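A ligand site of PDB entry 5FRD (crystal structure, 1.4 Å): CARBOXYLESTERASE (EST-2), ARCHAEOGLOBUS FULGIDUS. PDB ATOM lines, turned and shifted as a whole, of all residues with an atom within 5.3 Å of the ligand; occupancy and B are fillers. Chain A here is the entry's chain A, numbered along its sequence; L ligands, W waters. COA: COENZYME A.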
ATOM      1  N   SER A  89      -2.889  21.336  21.291  1.00  0.00           N
ATOM      2  CA  SER A  89      -2.535  21.866  19.956  1.00  0.00           C
ATOM      3  C   SER A  89      -2.232  20.750  18.944  1.00  0.00           C
ATOM      4  O   SER A  89      -3.156  19.974  18.691  1.00  0.00           O
ATOM      5  CB  SER A  89      -1.452  22.936  20.102  1.00  0.00           C
ATOM      6  OG  SER A  89      -1.509  23.853  18.986  1.00  0.00           O
ATOM      7  N   GLY A 115      -7.828  22.265  17.678  1.00  0.00           N
ATOM      8  CA  GLY A 115      -8.833  22.562  16.673  1.00  0.00           C
ATOM      9  C   GLY A 115      -9.039  21.388  15.745  1.00  0.00           C
ATOM     10  O   GLY A 115      -8.212  20.463  15.677  1.00  0.00           O
ATOM     11  N   ALA A 116     -10.142  21.431  15.027  1.00  0.00           N
ATOM     12  CA  ALA A 116     -10.427  20.460  13.962  1.00  0.00           C
ATOM     13  C   ALA A 116      -9.664  20.703  12.680  1.00  0.00           C
ATOM     14  O   ALA A 116      -9.588  19.845  11.823  1.00  0.00           O
ATOM     15  CB  ALA A 116     -11.920  20.465  13.680  1.00  0.00           C
ATOM     16  N   ARG A 117      -9.045  21.864  12.569  1.00  0.00           N
ATOM     17  CA  ARG A 117      -8.191  22.272  11.475  1.00  0.00           C
ATOM     18  C   ARG A 117      -7.175  23.243  12.071  1.00  0.00           C
ATOM     19  O   ARG A 117      -7.558  24.123  12.886  1.00  0.00           O
ATOM     20  CB  ARG A 117      -9.007  22.989  10.394  1.00  0.00           C
ATOM     21  CG  ARG A 117      -8.211  23.334   9.144  1.00  0.00           C
ATOM     22  CD  ARG A 117      -9.015  24.214   8.198  1.00  0.00           C
ATOM     23  NE  ARG A 117     -10.018  23.430   7.486  1.00  0.00           N
ATOM     24  CZ  ARG A 117     -10.875  23.929   6.606  1.00  0.00           C
ATOM     25  NH1 ARG A 117     -10.903  25.234   6.346  1.00  0.00           N
ATOM     26  NH2 ARG A 117     -11.743  23.109   6.026  1.00  0.00           N
ATOM     27  N   LEU A 118      -5.903  23.069  11.700  1.00  0.00           N
ATOM     28  CA  LEU A 118      -4.812  23.819  12.349  1.00  0.00           C
ATOM     29  C   LEU A 118      -3.893  24.501  11.361  1.00  0.00           C
ATOM     30  O   LEU A 118      -2.659  24.432  11.463  1.00  0.00           O
ATOM     31  CB  LEU A 118      -4.061  22.890  13.309  1.00  0.00           C
ATOM     32  CG  LEU A 118      -4.845  22.405  14.529  1.00  0.00           C
ATOM     33  CD1 LEU A 118      -4.021  21.369  15.286  1.00  0.00           C
ATOM     34  CD2 LEU A 118      -5.212  23.553  15.471  1.00  0.00           C
ATOM     35  N   ARG A 119      -4.485  25.252  10.437  1.00  0.00           N
ATOM     36  CA  ARG A 119      -3.694  26.083   9.563  1.00  0.00           C
ATOM     37  C   ARG A 119      -2.777  27.004  10.382  1.00  0.00           C
ATOM     38  O   ARG A 119      -3.181  27.539  11.419  1.00  0.00           O
ATOM     39  CB  ARG A 119      -4.595  26.923   8.670  1.00  0.00           C
ATOM     40  CG  ARG A 119      -5.302  26.129   7.569  1.00  0.00           C
ATOM     41  CD  ARG A 119      -4.377  25.640   6.453  1.00  0.00           C
ATOM     42  NE  ARG A 119      -3.433  26.654   6.024  1.00  0.00           N
ATOM     43  CZ  ARG A 119      -3.732  27.755   5.348  1.00  0.00           C
ATOM     44  NH1 ARG A 119      -4.973  27.982   4.934  1.00  0.00           N
ATOM     45  NH2 ARG A 119      -2.773  28.644   5.082  1.00  0.00           N
ATOM     46  N   VAL A 120      -1.568  27.190   9.875  1.00  0.00           N
ATOM     47  CA  VAL A 120      -0.572  28.025  10.522  1.00  0.00           C
ATOM     48  C   VAL A 120      -0.320  29.313   9.707  1.00  0.00           C
ATOM     49  O   VAL A 120      -0.139  29.255   8.484  1.00  0.00           O
ATOM     50  CB  VAL A 120       0.742  27.248  10.704  1.00  0.00           C
ATOM     51  CG1 VAL A 120       1.782  28.114  11.396  1.00  0.00           C
ATOM     52  CG2 VAL A 120       0.493  25.948  11.470  1.00  0.00           C
ATOM     53  N   LEU A 121      -0.291  30.428  10.399  1.00  0.00           N
ATOM     54  CA  LEU A 121       0.007  31.715   9.756  1.00  0.00           C
ATOM     55  C   LEU A 121       1.253  31.590   8.916  1.00  0.00           C
ATOM     56  O   LEU A 121       2.295  31.196   9.430  1.00  0.00           O
ATOM     57  CB  LEU A 121       0.298  32.786  10.799  1.00  0.00           C
ATOM     58  CG  LEU A 121      -0.851  33.468  11.518  1.00  0.00           C
ATOM     59  CD1 LEU A 121      -0.292  34.292  12.670  1.00  0.00           C
ATOM     60  CD2 LEU A 121      -1.660  34.315  10.546  1.00  0.00           C
ATOM     61  N   PRO A 122       1.173  31.917   7.599  1.00  0.00           N
ATOM     62  CA  PRO A 122       2.378  31.858   6.767  1.00  0.00           C
ATOM     63  C   PRO A 122       3.573  32.668   7.296  1.00  0.00           C
ATOM     64  O   PRO A 122       4.708  32.230   7.219  1.00  0.00           O
ATOM     65  CB  PRO A 122       1.882  32.390   5.426  1.00  0.00           C
ATOM     66  CG  PRO A 122       0.493  31.892   5.369  1.00  0.00           C
ATOM     67  CD  PRO A 122      -0.039  32.090   6.767  1.00  0.00           C
ATOM     68  N   ILE A 124       4.495  32.831  10.328  1.00  0.00           N
ATOM     69  CA  ILE A 124       5.192  31.929  11.258  1.00  0.00           C
ATOM     70  C   ILE A 124       5.852  30.834  10.436  1.00  0.00           C
ATOM     71  O   ILE A 124       7.037  30.622  10.542  1.00  0.00           O
ATOM     72  CB  ILE A 124       4.228  31.326  12.326  1.00  0.00           C
ATOM     73  CG1 ILE A 124       3.618  32.411  13.240  1.00  0.00           C
ATOM     74  CG2 ILE A 124       4.952  30.265  13.175  1.00  0.00           C
ATOM     75  CD1 ILE A 124       2.489  31.979  14.160  1.00  0.00           C
ATOM     76  N   MET A 142       1.285  35.115  20.589  1.00  0.00           N
ATOM     77  CA  MET A 142      -0.066  34.586  20.440  1.00  0.00           C
ATOM     78  C   MET A 142      -0.346  33.399  21.365  1.00  0.00           C
ATOM     79  O   MET A 142      -1.468  32.874  21.372  1.00  0.00           O
ATOM     80  CB  MET A 142      -0.252  34.136  18.986  1.00  0.00           C
ATOM     81  CG  MET A 142      -0.148  35.302  17.994  1.00  0.00           C
ATOM     82  SD  MET A 142      -0.051  34.832  16.268  1.00  0.00           S
ATOM     83  CE  MET A 142      -1.741  34.353  16.003  1.00  0.00           C
ATOM     84  N   LEU A 169       4.749  22.014  12.812  1.00  0.00           N
ATOM     85  CA  LEU A 169       3.783  23.007  12.348  1.00  0.00           C
ATOM     86  C   LEU A 169       3.341  22.699  10.924  1.00  0.00           C
ATOM     87  O   LEU A 169       2.189  22.990  10.577  1.00  0.00           O
ATOM     88  CB  LEU A 169       4.316  24.420  12.460  1.00  0.00           C
ATOM     89  CG  LEU A 169       4.463  24.931  13.887  1.00  0.00           C
ATOM     90  CD1 LEU A 169       5.159  26.294  13.849  1.00  0.00           C
ATOM     91  CD2 LEU A 169       3.128  25.066  14.594  1.00  0.00           C
ATOM     92  N   CYS A 172       0.622  20.232  11.356  1.00  0.00           N
ATOM     93  CA  CYS A 172      -0.581  20.984  11.747  1.00  0.00           C
ATOM     94  C   CYS A 172      -1.263  21.639  10.556  1.00  0.00           C
ATOM     95  O   CYS A 172      -2.516  21.588  10.393  1.00  0.00           O
ATOM     96  CB  CYS A 172      -0.263  22.080  12.767  1.00  0.00           C
ATOM     97  SG  CYS A 172       0.213  21.502  14.405  1.00  0.00           S
ATOM     98  N   LEU A 178     -12.341  19.354   9.602  1.00  0.00           N
ATOM     99  CA  LEU A 178     -13.422  20.315   9.894  1.00  0.00           C
ATOM    100  C   LEU A 178     -14.763  19.862   9.253  1.00  0.00           C
ATOM    101  O   LEU A 178     -15.784  19.810   9.931  1.00  0.00           O
ATOM    102  CB  LEU A 178     -13.014  21.710   9.424  1.00  0.00           C
ATOM    103  CG  LEU A 178     -13.870  22.893   9.824  1.00  0.00           C
ATOM    104  CD1 LEU A 178     -13.735  23.155  11.307  1.00  0.00           C
ATOM    105  CD2 LEU A 178     -13.449  24.136   9.026  1.00  0.00           C
ATOM    106  N   ARG A 182     -18.482  18.832  10.606  1.00  0.00           N
ATOM    107  CA  ARG A 182     -19.626  19.667  10.158  1.00  0.00           C
ATOM    108  C   ARG A 182     -20.742  18.812   9.562  1.00  0.00           C
ATOM    109  O   ARG A 182     -21.904  19.074   9.825  1.00  0.00           O
ATOM    110  CB  ARG A 182     -19.159  20.716   9.142  1.00  0.00           C
ATOM    111  CG  ARG A 182     -18.663  22.027   9.745  1.00  0.00           C
ATOM    112  CD  ARG A 182     -18.110  22.927   8.650  1.00  0.00           C
ATOM    113  NE  ARG A 182     -17.748  24.277   9.113  1.00  0.00           N
ATOM    114  CZ  ARG A 182     -16.989  25.151   8.455  1.00  0.00           C
ATOM    115  NH1 ARG A 182     -16.467  24.861   7.259  1.00  0.00           N
ATOM    116  NH2 ARG A 182     -16.746  26.350   8.989  1.00  0.00           N
ATOM    117  N   LYS A 201      -4.591  33.087  20.969  1.00  0.00           N
ATOM    118  CA  LYS A 201      -4.725  33.570  19.603  1.00  0.00           C
ATOM    119  C   LYS A 201      -4.276  32.561  18.554  1.00  0.00           C
ATOM    120  O   LYS A 201      -4.519  32.750  17.359  1.00  0.00           O
ATOM    121  CB  LYS A 201      -4.001  34.908  19.433  1.00  0.00           C
ATOM    122  CG  LYS A 201      -4.621  36.002  20.275  1.00  0.00           C
ATOM    123  CD  LYS A 201      -4.264  37.400  19.852  1.00  0.00           C
ATOM    124  CE  LYS A 201      -5.247  38.062  18.907  1.00  0.00           C
ATOM    125  NZ  LYS A 201      -4.569  39.090  18.069  1.00  0.00           N
ATOM    126  N   LEU A 202      -3.609  31.482  18.972  1.00  0.00           N
ATOM    127  CA  LEU A 202      -3.219  30.447  18.035  1.00  0.00           C
ATOM    128  C   LEU A 202      -4.391  29.517  17.736  1.00  0.00           C
ATOM    129  O   LEU A 202      -4.565  29.068  16.610  1.00  0.00           O
ATOM    130  CB  LEU A 202      -2.023  29.656  18.555  1.00  0.00           C
ATOM    131  CG  LEU A 202      -0.695  30.411  18.607  1.00  0.00           C
ATOM    132  CD1 LEU A 202       0.367  29.600  19.320  1.00  0.00           C
ATOM    133  CD2 LEU A 202      -0.258  30.754  17.176  1.00  0.00           C
ATOM    134  N   THR A 203      -5.120  29.159  18.791  1.00  0.00           N
ATOM    135  CA  THR A 203      -6.296  28.292  18.674  1.00  0.00           C
ATOM    136  C   THR A 203      -7.369  28.989  19.515  1.00  0.00           C
ATOM    137  O   THR A 203      -7.514  28.756  20.686  1.00  0.00           O
ATOM    138  CB  THR A 203      -6.010  26.855  19.181  1.00  0.00           C
ATOM    139  OG1 THR A 203      -5.471  26.886  20.492  1.00  0.00           O
ATOM    140  CG2 THR A 203      -5.034  26.141  18.292  1.00  0.00           C
ATOM    141  N   PRO A 204      -8.099  29.920  18.883  1.00  0.00           N
ATOM    142  CA  PRO A 204      -8.948  30.811  19.669  1.00  0.00           C
ATOM    143  C   PRO A 204     -10.257  30.176  20.127  1.00  0.00           C
ATOM    144  O   PRO A 204     -10.550  29.000  19.846  1.00  0.00           O
ATOM    145  CB  PRO A 204      -9.189  31.970  18.710  1.00  0.00           C
ATOM    146  CG  PRO A 204      -9.071  31.374  17.376  1.00  0.00           C
ATOM    147  CD  PRO A 204      -8.023  30.302  17.474  1.00  0.00           C
ATOM    148  N   LYS A 206     -13.306  30.335  19.151  1.00  0.00           N
ATOM    149  CA  LYS A 206     -14.186  29.718  18.157  1.00  0.00           C
ATOM    150  C   LYS A 206     -13.801  28.297  17.816  1.00  0.00           C
ATOM    151  O   LYS A 206     -14.671  27.509  17.512  1.00  0.00           O
ATOM    152  CB  LYS A 206     -14.314  30.530  16.901  1.00  0.00           C
ATOM    153  CG  LYS A 206     -15.137  31.797  17.074  1.00  0.00           C
ATOM    154  CD  LYS A 206     -14.986  32.699  15.844  1.00  0.00           C
ATOM    155  CE  LYS A 206     -15.473  34.136  16.110  1.00  0.00           C
ATOM    156  NZ  LYS A 206     -16.157  34.737  14.917  1.00  0.00           N
ATOM    157  N   TYR A 207     -12.503  27.960  17.874  1.00  0.00           N
ATOM    158  CA  TYR A 207     -12.115  26.578  17.594  1.00  0.00           C
ATOM    159  C   TYR A 207     -12.681  25.638  18.651  1.00  0.00           C
ATOM    160  O   TYR A 207     -13.015  24.465  18.373  1.00  0.00           O
ATOM    161  CB  TYR A 207     -10.618  26.400  17.571  1.00  0.00           C
ATOM    162  CG  TYR A 207      -9.846  27.014  16.429  1.00  0.00           C
ATOM    163  CD1 TYR A 207     -10.429  27.955  15.554  1.00  0.00           C
ATOM    164  CD2 TYR A 207      -8.517  26.653  16.202  1.00  0.00           C
ATOM    165  CE1 TYR A 207      -9.683  28.525  14.503  1.00  0.00           C
ATOM    166  CE2 TYR A 207      -7.772  27.224  15.173  1.00  0.00           C
ATOM    167  CZ  TYR A 207      -8.358  28.180  14.339  1.00  0.00           C
ATOM    168  OH  TYR A 207      -7.641  28.801  13.311  1.00  0.00           O
ATOM    169  N   PHE A 210     -16.412  25.309  18.465  1.00  0.00           N
ATOM    170  CA  PHE A 210     -16.715  24.392  17.347  1.00  0.00           C
ATOM    171  C   PHE A 210     -16.775  22.964  17.875  1.00  0.00           C
ATOM    172  O   PHE A 210     -17.747  22.232  17.631  1.00  0.00           O
ATOM    173  CB  PHE A 210     -15.694  24.512  16.241  1.00  0.00           C
ATOM    174  CG  PHE A 210     -15.928  23.546  15.111  1.00  0.00           C
ATOM    175  CD1 PHE A 210     -16.739  23.907  14.059  1.00  0.00           C
ATOM    176  CD2 PHE A 210     -15.364  22.288  15.117  1.00  0.00           C
ATOM    177  CE1 PHE A 210     -16.971  23.052  12.977  1.00  0.00           C
ATOM    178  CE2 PHE A 210     -15.612  21.400  14.053  1.00  0.00           C
ATOM    179  CZ  PHE A 210     -16.436  21.782  13.001  1.00  0.00           C
HETATM  180  N1A COA L   1     -12.487  25.458  14.034  1.00  0.00           N
HETATM  181  C2A COA L   1     -13.537  26.152  13.564  1.00  0.00           C
HETATM  182  N3A COA L   1     -13.450  26.867  12.431  1.00  0.00           N
HETATM  183  C4A COA L   1     -12.304  26.901  11.718  1.00  0.00           C
HETATM  184  C5A COA L   1     -11.127  26.185  12.162  1.00  0.00           C
HETATM  185  C6A COA L   1     -11.289  25.413  13.394  1.00  0.00           C
HETATM  186  N6A COA L   1     -10.230  24.725  13.877  1.00  0.00           N
HETATM  187  N7A COA L   1     -10.128  26.401  11.306  1.00  0.00           N
HETATM  188  C8A COA L   1     -10.643  27.185  10.338  1.00  0.00           C
HETATM  189  N9A COA L   1     -11.932  27.477  10.610  1.00  0.00           N
HETATM  190  C1B COA L   1     -12.789  28.355   9.774  1.00  0.00           C
HETATM  191  C2B COA L   1     -12.308  29.763   9.951  1.00  0.00           C
HETATM  192  O2B COA L   1     -12.895  30.344  11.114  1.00  0.00           O
HETATM  193  C3B COA L   1     -12.707  30.383   8.623  1.00  0.00           C
HETATM  194  O3B COA L   1     -14.076  30.769   8.677  1.00  0.00           O
HETATM  195  P3B COA L   1     -14.609  32.174   8.101  1.00  0.00           P
HETATM  196  O7A COA L   1     -14.306  32.030   6.617  1.00  0.00           O
HETATM  197  O8A COA L   1     -13.789  33.212   8.844  1.00  0.00           O
HETATM  198  O9A COA L   1     -16.077  32.181   8.474  1.00  0.00           O
HETATM  199  C4B COA L   1     -12.533  29.248   7.630  1.00  0.00           C
HETATM  200  O4B COA L   1     -12.624  28.037   8.406  1.00  0.00           O
HETATM  201  C5B COA L   1     -11.221  29.269   6.861  1.00  0.00           C
HETATM  202  O5B COA L   1     -10.129  29.262   7.793  1.00  0.00           O
HETATM  203  P1A COA L   1      -8.737  28.520   7.452  1.00  0.00           P
HETATM  204  O1A COA L   1      -8.978  27.191   6.862  1.00  0.00           O
HETATM  205  O2A COA L   1      -7.940  28.591   8.747  1.00  0.00           O
HETATM  206  O3A COA L   1      -8.002  29.368   6.293  1.00  0.00           O
HETATM  207  P2A COA L   1      -7.692  30.940   6.211  1.00  0.00           P
HETATM  208  O4A COA L   1      -6.861  31.009   4.949  1.00  0.00           O
HETATM  209  O5A COA L   1      -8.955  31.722   6.410  1.00  0.00           O
HETATM  210  O6A COA L   1      -6.784  31.336   7.489  1.00  0.00           O
HETATM  211  CBP COA L   1      -4.922  31.442   8.938  1.00  0.00           C
HETATM  212  CCP COA L   1      -5.472  30.830   7.659  1.00  0.00           C
HETATM  213  CDP COA L   1      -3.530  30.858   9.190  1.00  0.00           C
HETATM  214  CEP COA L   1      -4.826  32.970   8.747  1.00  0.00           C
HETATM  215  CAP COA L   1      -5.868  31.092  10.115  1.00  0.00           C
HETATM  216  OAP COA L   1      -6.078  29.657  10.176  1.00  0.00           O
HETATM  217  C9P COA L   1      -5.354  31.597  11.447  1.00  0.00           C
HETATM  218  O9P COA L   1      -5.325  32.783  11.679  1.00  0.00           O
HETATM  219  N8P COA L   1      -4.986  30.668  12.336  1.00  0.00           N
HETATM  220  C7P COA L   1      -4.612  30.967  13.727  1.00  0.00           C
HETATM  221  C6P COA L   1      -3.129  31.225  13.938  1.00  0.00           C
HETATM  222  C5P COA L   1      -2.180  30.045  13.841  1.00  0.00           C
HETATM  223  O5P COA L   1      -1.161  30.119  13.140  1.00  0.00           O
HETATM  224  N4P COA L   1      -2.462  28.965  14.573  1.00  0.00           N
HETATM  225  C3P COA L   1      -1.585  27.825  14.660  1.00  0.00           C
HETATM  226  C2P COA L   1      -2.402  26.566  14.814  1.00  0.00           C
HETATM  227  S1P COA L   1      -1.287  25.178  15.078  1.00  0.00           S
HETATM  228  O   HOH W   1      -5.613  27.301  12.601  1.00  0.00           O
HETATM  229  O   HOH W   2      -7.449  26.170   4.855  1.00  0.00           O
HETATM  230  O   HOH W   3      -7.332  34.577  10.932  1.00  0.00           O
HETATM  231  O   HOH W   4      -7.360  26.364  10.600  1.00  0.00           O
HETATM  232  O   HOH W   5      -9.018  29.784  11.114  1.00  0.00           O
HETATM  233  O   HOH W   6     -12.028  23.417  15.919  1.00  0.00           O
HETATM  234  O   HOH W   7      -4.206  34.658  13.395  1.00  0.00           O
HETATM  235  O   HOH W   8     -16.106  27.482  11.451  1.00  0.00           O
HETATM  236  O   HOH W   9     -14.545  26.532   6.471  1.00  0.00           O
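The backbone NH (N) of Ala 116 lies close to a nitrogen (N6A) of the ligand (3.5 Å).
Gly 115 touches the ligand.
Leu 118 touches the ligand.
Val 120 touches the ligand.
Met 142 touches the ligand (CE to C6P, 3.997 Å).
Cys 172 touches the ligand (CB to S1P, 3.998 Å).
Leu 178 touches the ligand.
O of Lys 201 touches C6P of the ligand, at 3.995 Å.
CB of Phe 210 touches C2A of the ligand, at 3.8 Å.
The backbone NH of Lys 201 is in hydrogen-bond range of the backbone carbonyl oxygen of Met 142.
Water W2 bridges O1A of the ligand (2.7 Å) and NH1 of Arg 119 (3.1 Å).
Water W6 lies within hydrogen-bond range of N1A of the ligand (2.8 Å), O of Tyr 207 (2.8 Å) and N of Ala 116 (2.9 Å).
Water W4 lies within hydrogen-bond range of a nitrogen (N7A) of the ligand, the backbone NH of Arg 119 and the backbone carbonyl oxygen of Arg 117.
Water W5 bridges OH of Tyr 207 and O2A of the ligand.
Water W9 bridges the guanidinium group (NH1) of Arg 182 (2.7 Å) and an oxygen (O4B) of the ligand (3.1 Å).
Water W1 lies within hydrogen-bond range of OH of Tyr 207 (2.6 Å), O of Arg 119 (2.7 Å) and OAP of the ligand (3.4 Å).
The backbone carbonyl oxygen (O) of Arg 117 sits at hydrogen-bond distance from a nitrogen (N6A) of the ligand (2.9 Å).
The guanidinium group of Arg 117 is in salt-bridge range of an oxygen (O1A) of the ligand.
O5P of the ligand is in hydrogen-bond range of N of Leu 121, at 2.9 Å.
O of Leu 202 is in hydrogen-bond range of N4P of the ligand (2.9 Å).
The side-chain hydroxyl (OH) of Tyr 207 sits at hydrogen-bond distance from a nitrogen (N8P) of the ligand.
An oxygen (O4A) of the ligand is in salt-bridge range of the guanidinium group of Arg 119 (3.6 Å).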
